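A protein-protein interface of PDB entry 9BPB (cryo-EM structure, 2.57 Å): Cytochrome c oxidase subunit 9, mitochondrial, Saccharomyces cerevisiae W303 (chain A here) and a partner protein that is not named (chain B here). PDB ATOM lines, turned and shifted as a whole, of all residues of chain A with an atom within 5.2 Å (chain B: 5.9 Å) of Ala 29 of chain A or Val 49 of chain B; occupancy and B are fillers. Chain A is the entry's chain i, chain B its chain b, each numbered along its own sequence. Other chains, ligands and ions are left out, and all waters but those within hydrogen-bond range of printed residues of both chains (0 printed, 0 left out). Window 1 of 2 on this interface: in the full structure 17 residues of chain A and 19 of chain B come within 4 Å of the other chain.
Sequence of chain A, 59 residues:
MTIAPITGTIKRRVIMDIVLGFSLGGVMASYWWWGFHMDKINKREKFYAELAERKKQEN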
ATOM      1  N   GLY A  21      15.927  33.609 -25.764  1.00  0.00           N
ATOM      2  CA  GLY A  21      15.780  32.259 -25.247  1.00  0.00           C
ATOM      3  C   GLY A  21      14.655  32.134 -24.238  1.00  0.00           C
ATOM      4  O   GLY A  21      13.919  31.145 -24.232  1.00  0.00           O
ATOM      5  N   PHE A  22      14.504  33.137 -23.374  1.00  0.00           N
ATOM      6  CA  PHE A  22      13.387  33.133 -22.436  1.00  0.00           C
ATOM      7  C   PHE A  22      12.073  33.425 -23.148  1.00  0.00           C
ATOM      8  O   PHE A  22      11.035  32.845 -22.806  1.00  0.00           O
ATOM      9  CB  PHE A  22      13.638  34.146 -21.322  1.00  0.00           C
ATOM     10  CG  PHE A  22      14.563  33.648 -20.251  1.00  0.00           C
ATOM     11  CD1 PHE A  22      14.109  32.786 -19.269  1.00  0.00           C
ATOM     12  CD2 PHE A  22      15.892  34.036 -20.231  1.00  0.00           C
ATOM     13  CE1 PHE A  22      14.960  32.327 -18.287  1.00  0.00           C
ATOM     14  CE2 PHE A  22      16.747  33.577 -19.250  1.00  0.00           C
ATOM     15  CZ  PHE A  22      16.280  32.725 -18.276  1.00  0.00           C
ATOM     16  N   GLY A  25      11.298  30.352 -25.270  1.00  0.00           N
ATOM     17  CA  GLY A  25      10.880  29.407 -24.255  1.00  0.00           C
ATOM     18  C   GLY A  25       9.627  29.825 -23.521  1.00  0.00           C
ATOM     19  O   GLY A  25       8.947  28.973 -22.940  1.00  0.00           O
ATOM     20  N   GLY A  26       9.309  31.121 -23.528  1.00  0.00           N
ATOM     21  CA  GLY A  26       8.066  31.571 -22.924  1.00  0.00           C
ATOM     22  C   GLY A  26       6.841  31.077 -23.668  1.00  0.00           C
ATOM     23  O   GLY A  26       5.868  30.632 -23.052  1.00  0.00           O
ATOM     24  N   VAL A  27       6.870  31.143 -25.001  1.00  0.00           N
ATOM     25  CA  VAL A  27       5.733  30.681 -25.793  1.00  0.00           C
ATOM     26  C   VAL A  27       5.590  29.169 -25.691  1.00  0.00           C
ATOM     27  O   VAL A  27       4.477  28.644 -25.569  1.00  0.00           O
ATOM     28  CB  VAL A  27       5.879  31.146 -27.253  1.00  0.00           C
ATOM     29  CG1 VAL A  27       4.973  30.342 -28.166  1.00  0.00           C
ATOM     30  CG2 VAL A  27       5.564  32.629 -27.367  1.00  0.00           C
ATOM     31  N   MET A  28       6.711  28.444 -25.735  1.00  0.00           N
ATOM     32  CA  MET A  28       6.667  26.998 -25.552  1.00  0.00           C
ATOM     33  C   MET A  28       6.030  26.640 -24.217  1.00  0.00           C
ATOM     34  O   MET A  28       5.168  25.755 -24.146  1.00  0.00           O
ATOM     35  CB  MET A  28       8.077  26.417 -25.642  1.00  0.00           C
ATOM     36  CG  MET A  28       8.757  26.637 -26.976  1.00  0.00           C
ATOM     37  SD  MET A  28      10.441  26.001 -27.014  1.00  0.00           S
ATOM     38  CE  MET A  28      10.998  26.635 -28.592  1.00  0.00           C
ATOM     39  N   ALA A  29       6.443  27.321 -23.147  1.00  0.00           N
ATOM     40  CA  ALA A  29       5.837  27.096 -21.840  1.00  0.00           C
ATOM     41  C   ALA A  29       4.381  27.540 -21.817  1.00  0.00           C
ATOM     42  O   ALA A  29       3.530  26.863 -21.226  1.00  0.00           O
ATOM     43  CB  ALA A  29       6.637  27.826 -20.765  1.00  0.00           C
ATOM     44  N   SER A  30       4.072  28.673 -22.454  1.00  0.00           N
ATOM     45  CA  SER A  30       2.722  29.225 -22.367  1.00  0.00           C
ATOM     46  C   SER A  30       1.737  28.429 -23.213  1.00  0.00           C
ATOM     47  O   SER A  30       0.560  28.311 -22.853  1.00  0.00           O
ATOM     48  CB  SER A  30       2.726  30.693 -22.787  1.00  0.00           C
ATOM     49  OG  SER A  30       3.621  31.442 -21.987  1.00  0.00           O
ATOM     50  N   TYR A  31       2.189  27.883 -24.344  1.00  0.00           N
ATOM     51  CA  TYR A  31       1.297  27.064 -25.157  1.00  0.00           C
ATOM     52  C   TYR A  31       0.953  25.760 -24.450  1.00  0.00           C
ATOM     53  O   TYR A  31      -0.152  25.232 -24.613  1.00  0.00           O
ATOM     54  CB  TYR A  31       1.923  26.782 -26.523  1.00  0.00           C
ATOM     55  CG  TYR A  31       1.030  25.946 -27.412  1.00  0.00           C
ATOM     56  CD1 TYR A  31      -0.114  26.490 -27.982  1.00  0.00           C
ATOM     57  CD2 TYR A  31       1.323  24.615 -27.673  1.00  0.00           C
ATOM     58  CE1 TYR A  31      -0.937  25.732 -28.791  1.00  0.00           C
ATOM     59  CE2 TYR A  31       0.504  23.850 -28.481  1.00  0.00           C
ATOM     60  CZ  TYR A  31      -0.624  24.414 -29.037  1.00  0.00           C
ATOM     61  OH  TYR A  31      -1.444  23.660 -29.843  1.00  0.00           O
ATOM     62  N   TRP A  32       1.891  25.214 -23.677  1.00  0.00           N
ATOM     63  CA  TRP A  32       1.595  24.014 -22.902  1.00  0.00           C
ATOM     64  C   TRP A  32       0.535  24.293 -21.847  1.00  0.00           C
ATOM     65  O   TRP A  32      -0.382  23.490 -21.644  1.00  0.00           O
ATOM     66  CB  TRP A  32       2.865  23.472 -22.246  1.00  0.00           C
ATOM     67  CG  TRP A  32       2.579  22.383 -21.248  1.00  0.00           C
ATOM     68  CD1 TRP A  32       2.476  22.520 -19.896  1.00  0.00           C
ATOM     69  CD2 TRP A  32       2.343  20.999 -21.530  1.00  0.00           C
ATOM     70  NE1 TRP A  32       2.195  21.307 -19.317  1.00  0.00           N
ATOM     71  CE2 TRP A  32       2.110  20.357 -20.299  1.00  0.00           C
ATOM     72  CE3 TRP A  32       2.310  20.240 -22.702  1.00  0.00           C
ATOM     73  CZ2 TRP A  32       1.850  18.994 -20.207  1.00  0.00           C
ATOM     74  CZ3 TRP A  32       2.052  18.886 -22.609  1.00  0.00           C
ATOM     75  CH2 TRP A  32       1.824  18.277 -21.370  1.00  0.00           C
ATOM     76  N   TRP A  33       0.644  25.433 -21.163  1.00  0.00           N
ATOM     77  CA  TRP A  33      -0.270  25.714 -20.062  1.00  0.00           C
ATOM     78  C   TRP A  33      -1.656  26.085 -20.575  1.00  0.00           C
ATOM     79  O   TRP A  33      -2.651  25.447 -20.212  1.00  0.00           O
ATOM     80  CB  TRP A  33       0.295  26.830 -19.181  1.00  0.00           C
ATOM     81  CG  TRP A  33      -0.496  27.060 -17.926  1.00  0.00           C
ATOM     82  CD1 TRP A  33      -1.374  28.076 -17.689  1.00  0.00           C
ATOM     83  CD2 TRP A  33      -0.480  26.259 -16.737  1.00  0.00           C
ATOM     84  NE1 TRP A  33      -1.908  27.957 -16.429  1.00  0.00           N
ATOM     85  CE2 TRP A  33      -1.375  26.850 -15.824  1.00  0.00           C
ATOM     86  CE3 TRP A  33       0.202  25.100 -16.357  1.00  0.00           C
ATOM     87  CZ2 TRP A  33      -1.603  26.322 -14.556  1.00  0.00           C
ATOM     88  CZ3 TRP A  33      -0.028  24.576 -15.096  1.00  0.00           C
ATOM     89  CH2 TRP A  33      -0.922  25.189 -14.212  1.00  0.00           C
ATOM     90  N   MET B  44       6.409  20.952 -15.699  1.00  0.00           N
ATOM     91  CA  MET B  44       6.609  20.995 -17.145  1.00  0.00           C
ATOM     92  C   MET B  44       6.425  22.392 -17.712  1.00  0.00           C
ATOM     93  O   MET B  44       6.926  22.676 -18.805  1.00  0.00           O
ATOM     94  CB  MET B  44       5.657  20.023 -17.844  1.00  0.00           C
ATOM     95  CG  MET B  44       6.236  18.636 -18.057  1.00  0.00           C
ATOM     96  SD  MET B  44       7.351  18.544 -19.473  1.00  0.00           S
ATOM     97  CE  MET B  44       6.318  19.220 -20.768  1.00  0.00           C
ATOM     98  N   PHE B  45       5.709  23.268 -17.008  1.00  0.00           N
ATOM     99  CA  PHE B  45       5.645  24.666 -17.417  1.00  0.00           C
ATOM    100  C   PHE B  45       7.016  25.319 -17.325  1.00  0.00           C
ATOM    101  O   PHE B  45       7.358  26.186 -18.136  1.00  0.00           O
ATOM    102  CB  PHE B  45       4.628  25.414 -16.556  1.00  0.00           C
ATOM    103  CG  PHE B  45       4.502  26.871 -16.890  1.00  0.00           C
ATOM    104  CD1 PHE B  45       3.855  27.277 -18.041  1.00  0.00           C
ATOM    105  CD2 PHE B  45       5.029  27.834 -16.050  1.00  0.00           C
ATOM    106  CE1 PHE B  45       3.737  28.618 -18.349  1.00  0.00           C
ATOM    107  CE2 PHE B  45       4.915  29.174 -16.352  1.00  0.00           C
ATOM    108  CZ  PHE B  45       4.268  29.567 -17.504  1.00  0.00           C
ATOM    109  N   TYR B  46       7.817  24.911 -16.343  1.00  0.00           N
ATOM    110  CA  TYR B  46       9.150  25.462 -16.158  1.00  0.00           C
ATOM    111  C   TYR B  46      10.238  24.621 -16.809  1.00  0.00           C
ATOM    112  O   TYR B  46      11.330  25.139 -17.066  1.00  0.00           O
ATOM    113  CB  TYR B  46       9.445  25.619 -14.666  1.00  0.00           C
ATOM    114  CG  TYR B  46       8.614  26.692 -14.002  1.00  0.00           C
ATOM    115  CD1 TYR B  46       8.463  27.939 -14.588  1.00  0.00           C
ATOM    116  CD2 TYR B  46       7.975  26.454 -12.795  1.00  0.00           C
ATOM    117  CE1 TYR B  46       7.703  28.921 -13.990  1.00  0.00           C
ATOM    118  CE2 TYR B  46       7.211  27.429 -12.189  1.00  0.00           C
ATOM    119  CZ  TYR B  46       7.079  28.660 -12.791  1.00  0.00           C
ATOM    120  OH  TYR B  46       6.318  29.634 -12.187  1.00  0.00           O
ATOM    121  N   LEU B  47      10.007  23.402 -17.127  1.00  0.00           N
ATOM    122  CA  LEU B  47      11.019  22.549 -17.797  1.00  0.00           C
ATOM    123  C   LEU B  47      11.186  23.030 -19.232  1.00  0.00           C
ATOM    124  O   LEU B  47      12.280  22.831 -19.781  1.00  0.00           O
ATOM    125  CB  LEU B  47      10.520  21.098 -17.795  1.00  0.00           C
ATOM    126  CG  LEU B  47      10.335  20.421 -16.438  1.00  0.00           C
ATOM    127  CD1 LEU B  47      10.269  18.908 -16.585  1.00  0.00           C
ATOM    128  CD2 LEU B  47      11.420  20.816 -15.451  1.00  0.00           C
ATOM    129  N   LEU B  48      10.108  23.642 -19.801  1.00  0.00           N
ATOM    130  CA  LEU B  48      10.168  24.033 -21.203  1.00  0.00           C
ATOM    131  C   LEU B  48      10.919  25.344 -21.404  1.00  0.00           C
ATOM    132  O   LEU B  48      11.495  25.563 -22.475  1.00  0.00           O
ATOM    133  CB  LEU B  48       8.755  24.131 -21.771  1.00  0.00           C
ATOM    134  CG  LEU B  48       8.082  22.787 -22.056  1.00  0.00           C
ATOM    135  CD1 LEU B  48       6.695  22.980 -22.642  1.00  0.00           C
ATOM    136  CD2 LEU B  48       8.942  21.965 -22.995  1.00  0.00           C
ATOM    137  N   VAL B  49      10.921  26.228 -20.406  1.00  0.00           N
ATOM    138  CA  VAL B  49      11.689  27.466 -20.521  1.00  0.00           C
ATOM    139  C   VAL B  49      13.180  27.162 -20.570  1.00  0.00           C
ATOM    140  O   VAL B  49      13.906  27.668 -21.433  1.00  0.00           O
ATOM    141  CB  VAL B  49      11.349  28.424 -19.366  1.00  0.00           C
ATOM    142  CG1 VAL B  49      12.053  29.753 -19.560  1.00  0.00           C
ATOM    143  CG2 VAL B  49       9.847  28.624 -19.268  1.00  0.00           C
ATOM    144  N   ILE B  50      13.657  26.329 -19.644  1.00  0.00           N
ATOM    145  CA  ILE B  50      15.057  25.916 -19.661  1.00  0.00           C
ATOM    146  C   ILE B  50      15.362  25.139 -20.932  1.00  0.00           C
ATOM    147  O   ILE B  50      16.407  25.335 -21.562  1.00  0.00           O
ATOM    148  CB  ILE B  50      15.385  25.090 -18.402  1.00  0.00           C
ATOM    149  CG1 ILE B  50      14.906  25.814 -17.142  1.00  0.00           C
ATOM    150  CG2 ILE B  50      16.877  24.810 -18.325  1.00  0.00           C
ATOM    151  CD1 ILE B  50      15.418  27.231 -17.011  1.00  0.00           C
ATOM    152  N   LEU B  51      14.456  24.240 -21.327  1.00  0.00           N
ATOM    153  CA  LEU B  51      14.622  23.523 -22.584  1.00  0.00           C
ATOM    154  C   LEU B  51      14.629  24.483 -23.764  1.00  0.00           C
ATOM    155  O   LEU B  51      15.389  24.296 -24.721  1.00  0.00           O
ATOM    156  CB  LEU B  51      13.517  22.480 -22.744  1.00  0.00           C
ATOM    157  CG  LEU B  51      13.467  21.727 -24.073  1.00  0.00           C
ATOM    158  CD1 LEU B  51      14.753  20.950 -24.305  1.00  0.00           C
ATOM    159  CD2 LEU B  51      12.264  20.802 -24.124  1.00  0.00           C
ATOM    160  N   GLY B  52      13.792  25.519 -23.714  1.00  0.00           N
ATOM    161  CA  GLY B  52      13.792  26.521 -24.765  1.00  0.00           C
ATOM    162  C   GLY B  52      14.979  27.459 -24.726  1.00  0.00           C
ATOM    163  O   GLY B  52      15.303  28.070 -25.748  1.00  0.00           O
ATOM    164  N   LEU B  53      15.638  27.586 -23.572  1.00  0.00           N
ATOM    165  CA  LEU B  53      16.776  28.495 -23.453  1.00  0.00           C
ATOM    166  C   LEU B  53      18.077  27.827 -23.882  1.00  0.00           C
ATOM    167  O   LEU B  53      18.816  28.367 -24.711  1.00  0.00           O
ATOM    168  CB  LEU B  53      16.894  29.006 -22.018  1.00  0.00           C
ATOM    169  CG  LEU B  53      18.107  29.894 -21.736  1.00  0.00           C
ATOM    170  CD1 LEU B  53      17.953  31.251 -22.403  1.00  0.00           C
ATOM    171  CD2 LEU B  53      18.325  30.047 -20.243  1.00  0.00           C
ATOM    172  N   VAL B  54      18.377  26.657 -23.316  1.00  0.00           N
ATOM    173  CA  VAL B  54      19.623  25.968 -23.642  1.00  0.00           C
ATOM    174  C   VAL B  54      19.646  25.590 -25.114  1.00  0.00           C
ATOM    175  O   VAL B  54      20.670  25.736 -25.794  1.00  0.00           O
ATOM    176  CB  VAL B  54      19.804  24.734 -22.739  1.00  0.00           C
ATOM    177  CG1 VAL B  54      21.122  24.038 -23.050  1.00  0.00           C
ATOM    178  CG2 VAL B  54      19.733  25.131 -21.277  1.00  0.00           C
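Among the printed residues, merely in contact across the chains: Gly 21 of chain A with Gly 52 of chain B (3.7 Å), Gly 21 of chain A with Leu 53 of chain B (3.7 Å), Phe 22 of chain A with Val 49 of chain B (3.7 Å), Phe 22 of chain A with Leu 53 of chain B (3.9 Å), Gly 25 of chain A with Val 49 of chain B (3.8 Å), Met 28 of chain A with Leu 48 of chain B (3.5 Å), Ala 29 of chain A with Phe 45 of chain B (3.2 Å), Ala 29 of chain A with Val 49 of chain B (3.6 Å), Trp 32 of chain A with Met 44 of chain B (3.98 Å), Trp 32 of chain A with Leu 48 of chain B (3.9 Å) and Trp 33 of chain A with Phe 45 of chain B (3.8 Å).
Of the 11 printed residues of chain A, 7 touch a printed residue of chain B. Printed residues of chain A that touch a printed residue of chain B: Gly 21, Phe 22, Gly 25, Met 28, Ala 29, Trp 32 and Trp 33. Hydrophobic or aromatic side chains of chain A within 4 Å of the printed part of chain B: Phe 22, Ala 29, Trp 32 and Trp 33. Of the 11 printed residues of chain B, 6 touch a printed residue of chain A. Printed residues of chain B that touch a printed residue of chain A: Met 44, Phe 45, Leu 48, Val 49, Gly 52 and Leu 53. Hydrophobic or aromatic side chains of chain B that line the printed part of chain A: Met 44, Phe 45, Leu 48, Val 49 and Leu 53. Along chain B the printed residues that touch a printed residue of chain A span positions 44 to 53. Among the printed residues, 11 pairs touch across the chains. Among the printed residues, no Asp or Glu carboxylate lies within 4 Å of a Lys or Arg side-chain nitrogen of the other chain.
Of chain B, only Phe 45 and Val 49 come within 4 Å of Ala 29 of chain A. Of chain A, only Phe 22 (3.7 Å), Gly 25 (3.8 Å) and Ala 29 (3.6 Å) come within 4 Å of Val 49 of chain B. Of the printed residues of chain B, Trp 33 of chain A touches Phe 45 (3.8 Å). Printed residues of chain B within 4 Å of Trp 32 of chain A: Met 44 (3.98 Å) and Leu 48 (3.9 Å). Printed residues of chain A within 4 Å of Phe 45 of chain B: Ala 29 (3.2 Å) and Trp 33 (3.8 Å). Of the printed residues of chain B, Gly 21 of chain A touches Gly 52 (3.7 Å) and Leu 53 (3.7 Å). Of the printed residues of chain A, Leu 53 of chain B touches Gly 21 and Phe 22. Gly 26 of chain A touches none of the printed residues of chain B. Leu 51 of chain B touches none of the printed residues of chain A. The nearest printed residue of chain A that does not touch Leu 48 of chain B is Ala 29 of chain A (4.2 Å).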
